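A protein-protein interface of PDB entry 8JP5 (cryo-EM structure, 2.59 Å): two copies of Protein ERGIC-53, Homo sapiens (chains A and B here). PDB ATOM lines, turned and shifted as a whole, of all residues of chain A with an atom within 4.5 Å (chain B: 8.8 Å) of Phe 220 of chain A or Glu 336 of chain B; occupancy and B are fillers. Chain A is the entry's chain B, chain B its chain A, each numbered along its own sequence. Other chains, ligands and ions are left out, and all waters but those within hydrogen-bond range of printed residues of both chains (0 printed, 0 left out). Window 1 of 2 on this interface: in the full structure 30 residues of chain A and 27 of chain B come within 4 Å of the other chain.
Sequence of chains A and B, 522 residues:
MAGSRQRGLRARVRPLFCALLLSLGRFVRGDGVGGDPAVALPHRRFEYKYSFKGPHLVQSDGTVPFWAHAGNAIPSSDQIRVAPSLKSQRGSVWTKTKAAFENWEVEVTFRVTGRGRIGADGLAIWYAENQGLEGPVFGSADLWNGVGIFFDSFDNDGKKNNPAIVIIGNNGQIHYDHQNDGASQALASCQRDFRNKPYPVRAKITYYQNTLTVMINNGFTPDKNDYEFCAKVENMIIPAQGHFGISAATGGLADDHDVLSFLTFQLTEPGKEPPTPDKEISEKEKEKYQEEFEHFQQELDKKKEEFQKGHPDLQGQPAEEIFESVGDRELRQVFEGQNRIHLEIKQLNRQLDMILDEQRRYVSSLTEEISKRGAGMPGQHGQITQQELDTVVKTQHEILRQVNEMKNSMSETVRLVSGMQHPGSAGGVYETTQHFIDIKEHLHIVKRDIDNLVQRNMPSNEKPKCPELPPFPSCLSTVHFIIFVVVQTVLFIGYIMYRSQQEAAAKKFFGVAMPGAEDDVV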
ATOM      1  N   ASP A 193      29.755  19.057  -3.373  1.00  0.00           N
ATOM      2  CA  ASP A 193      28.317  19.003  -3.597  1.00  0.00           C
ATOM      3  C   ASP A 193      27.687  17.999  -2.643  1.00  0.00           C
ATOM      4  O   ASP A 193      28.163  16.864  -2.525  1.00  0.00           O
ATOM      5  CB  ASP A 193      28.001  18.627  -5.045  1.00  0.00           C
ATOM      6  CG  ASP A 193      26.618  19.076  -5.474  1.00  0.00           C
ATOM      7  OD1 ASP A 193      26.034  19.943  -4.791  1.00  0.00           O
ATOM      8  OD2 ASP A 193      26.113  18.562  -6.494  1.00  0.00           O
ATOM      9  N   LYS A 197      22.202  13.599  -3.419  1.00  0.00           N
ATOM     10  CA  LYS A 197      23.070  12.439  -3.515  1.00  0.00           C
ATOM     11  C   LYS A 197      22.262  11.156  -3.318  1.00  0.00           C
ATOM     12  O   LYS A 197      21.261  11.151  -2.596  1.00  0.00           O
ATOM     13  CB  LYS A 197      24.183  12.522  -2.476  1.00  0.00           C
ATOM     14  CG  LYS A 197      25.205  13.611  -2.763  1.00  0.00           C
ATOM     15  CD  LYS A 197      25.926  13.351  -4.077  1.00  0.00           C
ATOM     16  CE  LYS A 197      26.838  14.509  -4.447  1.00  0.00           C
ATOM     17  NZ  LYS A 197      26.066  15.711  -4.865  1.00  0.00           N
ATOM     18  N   PRO A 198      22.670  10.055  -3.959  1.00  0.00           N
ATOM     19  CA  PRO A 198      21.929   8.793  -3.796  1.00  0.00           C
ATOM     20  C   PRO A 198      21.981   8.223  -2.388  1.00  0.00           C
ATOM     21  O   PRO A 198      21.120   7.403  -2.042  1.00  0.00           O
ATOM     22  CB  PRO A 198      22.608   7.856  -4.802  1.00  0.00           C
ATOM     23  CG  PRO A 198      23.982   8.417  -4.965  1.00  0.00           C
ATOM     24  CD  PRO A 198      23.804   9.906  -4.890  1.00  0.00           C
ATOM     25  N   TYR A 199      22.946   8.620  -1.574  1.00  0.00           N
ATOM     26  CA  TYR A 199      23.103   8.142  -0.211  1.00  0.00           C
ATOM     27  C   TYR A 199      23.261   9.335   0.716  1.00  0.00           C
ATOM     28  O   TYR A 199      23.676  10.415   0.281  1.00  0.00           O
ATOM     29  CB  TYR A 199      24.316   7.206  -0.096  1.00  0.00           C
ATOM     30  CG  TYR A 199      24.194   5.960  -0.944  1.00  0.00           C
ATOM     31  CD1 TYR A 199      23.328   4.935  -0.585  1.00  0.00           C
ATOM     32  CD2 TYR A 199      24.941   5.810  -2.105  1.00  0.00           C
ATOM     33  CE1 TYR A 199      23.210   3.795  -1.357  1.00  0.00           C
ATOM     34  CE2 TYR A 199      24.831   4.672  -2.884  1.00  0.00           C
ATOM     35  CZ  TYR A 199      23.964   3.668  -2.504  1.00  0.00           C
ATOM     36  OH  TYR A 199      23.850   2.534  -3.276  1.00  0.00           O
ATOM     37  N   ASN A 218      31.211  12.134   0.357  1.00  0.00           N
ATOM     38  CA  ASN A 218      30.517  12.711  -0.791  1.00  0.00           C
ATOM     39  C   ASN A 218      29.104  12.166  -0.964  1.00  0.00           C
ATOM     40  O   ASN A 218      28.303  12.780  -1.676  1.00  0.00           O
ATOM     41  CB  ASN A 218      31.326  12.477  -2.067  1.00  0.00           C
ATOM     42  CG  ASN A 218      31.978  11.110  -2.103  1.00  0.00           C
ATOM     43  OD1 ASN A 218      31.619  10.218  -1.335  1.00  0.00           O
ATOM     44  ND2 ASN A 218      32.947  10.939  -2.994  1.00  0.00           N
ATOM     45  N   GLY A 219      28.780  11.039  -0.338  1.00  0.00           N
ATOM     46  CA  GLY A 219      27.440  10.497  -0.411  1.00  0.00           C
ATOM     47  C   GLY A 219      27.169   9.593  -1.590  1.00  0.00           C
ATOM     48  O   GLY A 219      25.999   9.326  -1.887  1.00  0.00           O
ATOM     49  N   PHE A 220      28.203   9.126  -2.282  1.00  0.00           N
ATOM     50  CA  PHE A 220      28.038   8.200  -3.393  1.00  0.00           C
ATOM     51  C   PHE A 220      28.165   6.742  -2.972  1.00  0.00           C
ATOM     52  O   PHE A 220      27.988   5.852  -3.810  1.00  0.00           O
ATOM     53  CB  PHE A 220      29.057   8.511  -4.494  1.00  0.00           C
ATOM     54  CG  PHE A 220      28.691   9.700  -5.337  1.00  0.00           C
ATOM     55  CD1 PHE A 220      27.528   9.700  -6.089  1.00  0.00           C
ATOM     56  CD2 PHE A 220      29.508  10.818  -5.373  1.00  0.00           C
ATOM     57  CE1 PHE A 220      27.187  10.792  -6.864  1.00  0.00           C
ATOM     58  CE2 PHE A 220      29.173  11.914  -6.147  1.00  0.00           C
ATOM     59  CZ  PHE A 220      28.011  11.901  -6.893  1.00  0.00           C
ATOM     60  N   THR A 221      28.464   6.476  -1.701  1.00  0.00           N
ATOM     61  CA  THR A 221      28.607   5.124  -1.190  1.00  0.00           C
ATOM     62  C   THR A 221      27.875   4.993   0.139  1.00  0.00           C
ATOM     63  O   THR A 221      27.837   5.948   0.925  1.00  0.00           O
ATOM     64  CB  THR A 221      30.090   4.759  -1.010  1.00  0.00           C
ATOM     65  OG1 THR A 221      30.206   3.584  -0.198  1.00  0.00           O
ATOM     66  CG2 THR A 221      30.850   5.904  -0.355  1.00  0.00           C
ATOM     67  N   PHE A 335      26.358   2.147  -9.077  1.00  0.00           N
ATOM     68  CA  PHE A 335      27.069   2.880  -8.034  1.00  0.00           C
ATOM     69  C   PHE A 335      28.125   2.018  -7.351  1.00  0.00           C
ATOM     70  O   PHE A 335      29.205   2.517  -7.014  1.00  0.00           O
ATOM     71  CB  PHE A 335      26.078   3.426  -7.008  1.00  0.00           C
ATOM     72  CG  PHE A 335      25.366   4.665  -7.463  1.00  0.00           C
ATOM     73  CD1 PHE A 335      26.066   5.698  -8.063  1.00  0.00           C
ATOM     74  CD2 PHE A 335      23.996   4.790  -7.306  1.00  0.00           C
ATOM     75  CE1 PHE A 335      25.416   6.841  -8.488  1.00  0.00           C
ATOM     76  CE2 PHE A 335      23.340   5.929  -7.732  1.00  0.00           C
ATOM     77  CZ  PHE A 335      24.051   6.954  -8.323  1.00  0.00           C
ATOM     78  N   GLU B 324      12.866  18.477 -13.055  1.00  0.00           N
ATOM     79  CA  GLU B 324      13.789  17.469 -13.556  1.00  0.00           C
ATOM     80  C   GLU B 324      13.169  16.102 -13.320  1.00  0.00           C
ATOM     81  O   GLU B 324      12.637  15.843 -12.236  1.00  0.00           O
ATOM     82  CB  GLU B 324      15.156  17.567 -12.869  1.00  0.00           C
ATOM     83  CG  GLU B 324      16.195  16.601 -13.420  1.00  0.00           C
ATOM     84  CD  GLU B 324      17.508  16.656 -12.663  1.00  0.00           C
ATOM     85  OE1 GLU B 324      17.607  17.441 -11.697  1.00  0.00           O
ATOM     86  OE2 GLU B 324      18.441  15.913 -13.034  1.00  0.00           O
ATOM     87  N   ARG B 329      17.471  12.377 -13.080  1.00  0.00           N
ATOM     88  CA  ARG B 329      18.251  12.568 -11.862  1.00  0.00           C
ATOM     89  C   ARG B 329      19.114  11.345 -11.588  1.00  0.00           C
ATOM     90  O   ARG B 329      20.319  11.464 -11.328  1.00  0.00           O
ATOM     91  CB  ARG B 329      17.321  12.848 -10.681  1.00  0.00           C
ATOM     92  CG  ARG B 329      18.012  12.833  -9.327  1.00  0.00           C
ATOM     93  CD  ARG B 329      17.392  13.840  -8.368  1.00  0.00           C
ATOM     94  NE  ARG B 329      17.727  15.217  -8.712  1.00  0.00           N
ATOM     95  CZ  ARG B 329      16.833  16.173  -8.923  1.00  0.00           C
ATOM     96  NH1 ARG B 329      15.535  15.936  -8.837  1.00  0.00           N
ATOM     97  NH2 ARG B 329      17.252  17.398  -9.228  1.00  0.00           N
ATOM     98  N   GLU B 330      18.526  10.151 -11.722  1.00  0.00           N
ATOM     99  CA  GLU B 330      19.273   8.914 -11.532  1.00  0.00           C
ATOM    100  C   GLU B 330      20.381   8.754 -12.563  1.00  0.00           C
ATOM    101  O   GLU B 330      21.299   7.955 -12.351  1.00  0.00           O
ATOM    102  CB  GLU B 330      18.327   7.714 -11.585  1.00  0.00           C
ATOM    103  CG  GLU B 330      17.314   7.679 -10.452  1.00  0.00           C
ATOM    104  CD  GLU B 330      16.476   6.416 -10.454  1.00  0.00           C
ATOM    105  OE1 GLU B 330      16.712   5.545 -11.318  1.00  0.00           O
ATOM    106  OE2 GLU B 330      15.582   6.295  -9.591  1.00  0.00           O
ATOM    107  N   LEU B 331      20.319   9.495 -13.668  1.00  0.00           N
ATOM    108  CA  LEU B 331      21.450   9.547 -14.582  1.00  0.00           C
ATOM    109  C   LEU B 331      22.479  10.581 -14.145  1.00  0.00           C
ATOM    110  O   LEU B 331      23.682  10.287 -14.142  1.00  0.00           O
ATOM    111  CB  LEU B 331      20.968   9.855 -16.003  1.00  0.00           C
ATOM    112  CG  LEU B 331      20.632   8.658 -16.894  1.00  0.00           C
ATOM    113  CD1 LEU B 331      20.670   9.061 -18.358  1.00  0.00           C
ATOM    114  CD2 LEU B 331      21.579   7.494 -16.635  1.00  0.00           C
ATOM    115  N   ARG B 332      22.017  11.770 -13.736  1.00  0.00           N
ATOM    116  CA  ARG B 332      22.931  12.882 -13.485  1.00  0.00           C
ATOM    117  C   ARG B 332      23.907  12.552 -12.365  1.00  0.00           C
ATOM    118  O   ARG B 332      25.117  12.779 -12.501  1.00  0.00           O
ATOM    119  CB  ARG B 332      22.143  14.147 -13.146  1.00  0.00           C
ATOM    120  CG  ARG B 332      22.924  15.433 -13.362  1.00  0.00           C
ATOM    121  CD  ARG B 332      22.007  16.646 -13.366  1.00  0.00           C
ATOM    122  NE  ARG B 332      21.068  16.625 -12.251  1.00  0.00           N
ATOM    123  CZ  ARG B 332      21.363  17.001 -11.014  1.00  0.00           C
ATOM    124  NH1 ARG B 332      22.570  17.443 -10.695  1.00  0.00           N
ATOM    125  NH2 ARG B 332      20.426  16.935 -10.074  1.00  0.00           N
ATOM    126  N   GLN B 333      23.399  11.982 -11.268  1.00  0.00           N
ATOM    127  CA  GLN B 333      24.262  11.545 -10.175  1.00  0.00           C
ATOM    128  C   GLN B 333      25.317  10.569 -10.674  1.00  0.00           C
ATOM    129  O   GLN B 333      26.496  10.683 -10.314  1.00  0.00           O
ATOM    130  CB  GLN B 333      23.420  10.902  -9.074  1.00  0.00           C
ATOM    131  CG  GLN B 333      22.269  11.761  -8.581  1.00  0.00           C
ATOM    132  CD  GLN B 333      21.238  10.959  -7.813  1.00  0.00           C
ATOM    133  OE1 GLN B 333      20.626  10.036  -8.351  1.00  0.00           O
ATOM    134  NE2 GLN B 333      21.043  11.304  -6.546  1.00  0.00           N
ATOM    135  N   VAL B 334      24.915   9.631 -11.539  1.00  0.00           N
ATOM    136  CA  VAL B 334      25.864   8.690 -12.125  1.00  0.00           C
ATOM    137  C   VAL B 334      26.953   9.447 -12.874  1.00  0.00           C
ATOM    138  O   VAL B 334      28.149   9.163 -12.719  1.00  0.00           O
ATOM    139  CB  VAL B 334      25.132   7.688 -13.039  1.00  0.00           C
ATOM    140  CG1 VAL B 334      26.110   6.999 -13.982  1.00  0.00           C
ATOM    141  CG2 VAL B 334      24.381   6.663 -12.204  1.00  0.00           C
ATOM    142  N   PHE B 335      26.554  10.458 -13.652  1.00  0.00           N
ATOM    143  CA  PHE B 335      27.534  11.299 -14.331  1.00  0.00           C
ATOM    144  C   PHE B 335      28.446  11.979 -13.320  1.00  0.00           C
ATOM    145  O   PHE B 335      29.672  12.006 -13.498  1.00  0.00           O
ATOM    146  CB  PHE B 335      26.824  12.333 -15.204  1.00  0.00           C
ATOM    147  CG  PHE B 335      27.755  13.169 -16.037  1.00  0.00           C
ATOM    148  CD1 PHE B 335      28.861  12.601 -16.646  1.00  0.00           C
ATOM    149  CD2 PHE B 335      27.521  14.523 -16.212  1.00  0.00           C
ATOM    150  CE1 PHE B 335      29.719  13.368 -17.415  1.00  0.00           C
ATOM    151  CE2 PHE B 335      28.374  15.295 -16.978  1.00  0.00           C
ATOM    152  CZ  PHE B 335      29.474  14.716 -17.581  1.00  0.00           C
ATOM    153  N   GLU B 336      27.869  12.485 -12.225  1.00  0.00           N
ATOM    154  CA  GLU B 336      28.684  13.068 -11.165  1.00  0.00           C
ATOM    155  C   GLU B 336      29.606  12.022 -10.558  1.00  0.00           C
ATOM    156  O   GLU B 336      30.763  12.317 -10.230  1.00  0.00           O
ATOM    157  CB  GLU B 336      27.788  13.693 -10.096  1.00  0.00           C
ATOM    158  CG  GLU B 336      26.958  14.866 -10.598  1.00  0.00           C
ATOM    159  CD  GLU B 336      26.419  15.725  -9.472  1.00  0.00           C
ATOM    160  OE1 GLU B 336      26.621  15.362  -8.293  1.00  0.00           O
ATOM    161  OE2 GLU B 336      25.790  16.765  -9.764  1.00  0.00           O
ATOM    162  N   GLY B 337      29.122  10.779 -10.445  1.00  0.00           N
ATOM    163  CA  GLY B 337      29.964   9.707  -9.944  1.00  0.00           C
ATOM    164  C   GLY B 337      31.174   9.451 -10.819  1.00  0.00           C
ATOM    165  O   GLY B 337      32.183   8.919 -10.351  1.00  0.00           O
ATOM    166  N   GLN B 338      31.091   9.821 -12.098  1.00  0.00           N
ATOM    167  CA  GLN B 338      32.260   9.724 -12.961  1.00  0.00           C
ATOM    168  C   GLN B 338      33.240  10.862 -12.702  1.00  0.00           C
ATOM    169  O   GLN B 338      34.458  10.650 -12.725  1.00  0.00           O
ATOM    170  CB  GLN B 338      31.823   9.703 -14.424  1.00  0.00           C
ATOM    171  CG  GLN B 338      30.982   8.489 -14.776  1.00  0.00           C
ATOM    172  CD  GLN B 338      30.473   8.522 -16.199  1.00  0.00           C
ATOM    173  OE1 GLN B 338      30.621   9.520 -16.903  1.00  0.00           O
ATOM    174  NE2 GLN B 338      29.862   7.426 -16.629  1.00  0.00           N
ATOM    175  N   ASN B 339      32.723  12.065 -12.420  1.00  0.00           N
ATOM    176  CA  ASN B 339      33.580  13.241 -12.298  1.00  0.00           C
ATOM    177  C   ASN B 339      34.539  13.144 -11.120  1.00  0.00           C
ATOM    178  O   ASN B 339      35.604  13.771 -11.148  1.00  0.00           O
ATOM    179  CB  ASN B 339      32.729  14.505 -12.177  1.00  0.00           C
ATOM    180  CG  ASN B 339      31.935  14.795 -13.436  1.00  0.00           C
ATOM    181  OD1 ASN B 339      32.499  14.921 -14.523  1.00  0.00           O
ATOM    182  ND2 ASN B 339      30.619  14.905 -13.295  1.00  0.00           N
ATOM    183  N   ARG B 340      34.186  12.377 -10.089  1.00  0.00           N
ATOM    184  CA  ARG B 340      35.140  12.071  -9.030  1.00  0.00           C
ATOM    185  C   ARG B 340      36.275  11.199  -9.557  1.00  0.00           C
ATOM    186  O   ARG B 340      37.457  11.533  -9.388  1.00  0.00           O
ATOM    187  CB  ARG B 340      34.419  11.377  -7.875  1.00  0.00           C
ATOM    188  CG  ARG B 340      35.333  10.698  -6.874  1.00  0.00           C
ATOM    189  CD  ARG B 340      34.535   9.768  -5.977  1.00  0.00           C
ATOM    190  NE  ARG B 340      33.504   9.064  -6.730  1.00  0.00           N
ATOM    191  CZ  ARG B 340      32.916   7.944  -6.333  1.00  0.00           C
ATOM    192  NH1 ARG B 340      33.233   7.365  -5.187  1.00  0.00           N
ATOM    193  NH2 ARG B 340      31.989   7.389  -7.109  1.00  0.00           N
ATOM    194  N   ILE B 341      35.925  10.103 -10.241  1.00  0.00           N
ATOM    195  CA  ILE B 341      36.909   9.102 -10.655  1.00  0.00           C
ATOM    196  C   ILE B 341      37.958   9.727 -11.563  1.00  0.00           C
ATOM    197  O   ILE B 341      39.162   9.466 -11.415  1.00  0.00           O
ATOM    198  CB  ILE B 341      36.201   7.915 -11.338  1.00  0.00           C
ATOM    199  CG1 ILE B 341      35.391   7.113 -10.317  1.00  0.00           C
ATOM    200  CG2 ILE B 341      37.200   7.020 -12.056  1.00  0.00           C
ATOM    201  CD1 ILE B 341      34.317   6.244 -10.938  1.00  0.00           C
ATOM    202  N   HIS B 342      37.516  10.591 -12.483  1.00  0.00           N
ATOM    203  CA  HIS B 342      38.418  11.303 -13.383  1.00  0.00           C
ATOM    204  C   HIS B 342      39.538  11.988 -12.611  1.00  0.00           C
ATOM    205  O   HIS B 342      40.718  11.867 -12.967  1.00  0.00           O
ATOM    206  CB  HIS B 342      37.629  12.333 -14.192  1.00  0.00           C
ATOM    207  CG  HIS B 342      37.011  11.787 -15.440  1.00  0.00           C
ATOM    208  ND1 HIS B 342      35.655  11.840 -15.682  1.00  0.00           N
ATOM    209  CD2 HIS B 342      37.563  11.190 -16.522  1.00  0.00           C
ATOM    210  CE1 HIS B 342      35.398  11.291 -16.855  1.00  0.00           C
ATOM    211  NE2 HIS B 342      36.538  10.890 -17.388  1.00  0.00           N
ATOM    212  N   LEU B 343      39.183  12.672 -11.516  1.00  0.00           N
ATOM    213  CA  LEU B 343      40.187  13.365 -10.716  1.00  0.00           C
ATOM    214  C   LEU B 343      41.224  12.387 -10.183  1.00  0.00           C
ATOM    215  O   LEU B 343      42.434  12.629 -10.283  1.00  0.00           O
ATOM    216  CB  LEU B 343      39.515  14.116  -9.566  1.00  0.00           C
ATOM    217  CG  LEU B 343      39.280  15.619  -9.738  1.00  0.00           C
ATOM    218  CD1 LEU B 343      38.243  15.896 -10.817  1.00  0.00           C
ATOM    219  CD2 LEU B 343      38.869  16.248  -8.415  1.00  0.00           C
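Hydrophobic or aromatic side chains of chain B that line the printed part of chain A: Val 334.
Among the printed residues, pairs that only touch across the chains: Asp 193 of chain A with Glu 336 of chain B (3.7 Å), Lys 197 of chain A with Gln 333 of chain B (3.5 Å), Asn 218 of chain A with Arg 340 of chain B (3.6 Å), Phe 220 of chain A with Gln 333 of chain B (3.5 Å), Phe 220 of chain A with Glu 336 of chain B (3.7 Å), Phe 220 of chain A with Gly 337 of chain B (3.9 Å) and Phe 335 of chain A with Val 334 of chain B (3.9 Å).
OD2 of Asp 193 of chain A lies within salt-bridge range of NZ of Lys 197 of chain A, 3.3 Å away. The backbone carbonyl oxygen (O) of Arg 329 of chain B sits close to the side-chain amide oxygen (OE1) of Gln 333 of chain B, at 3.3 Å. The side-chain carboxylate (OE2) of Glu 336 of chain B is in salt-bridge range of the guanidinium group (NH1) of Arg 332 of chain B (3.4 Å).
N of Pro 198 of chain A sits close to NE2 of Gln 333 of chain B (3.3 Å). The side-chain carboxylate (OE1) of Glu 336 of chain B lies within salt-bridge range of the side-chain amino group (NZ) of Lys 197 of chain A.
Of chain B, only Gln 333, Glu 336 and Gly 337 come within 4 Å of Phe 220 of chain A. Of chain A, only Asp 193, Lys 197 and Phe 220 come within 4 Å of Glu 336 of chain B. Gly 219 of chain A touches none of the printed residues of chain B. No residue of chain B comes within 4 Å of Thr 221 of chain A. Of the printed residues of chain A, Gln 333 of chain B touches Lys 197, Pro 198 and Phe 220. Printed residues of chain B within 4 Å of Lys 197 of chain A: Gln 333 (3.5 Å) and Glu 336 (3.5 Å). Of the printed residues of chain A, Arg 340 of chain B touches Asn 218. Of the printed residues of chain B, Asn 218 of chain A touches Arg 340. Arg 329 of chain B touches none of the printed residues of chain A. Tyr 199 of chain A touches none of the printed residues of chain B. The nearest printed residue of chain A that does not touch Glu 336 of chain B is Phe 335 of chain A (7.0 Å).
Position printed for both chains: 335.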
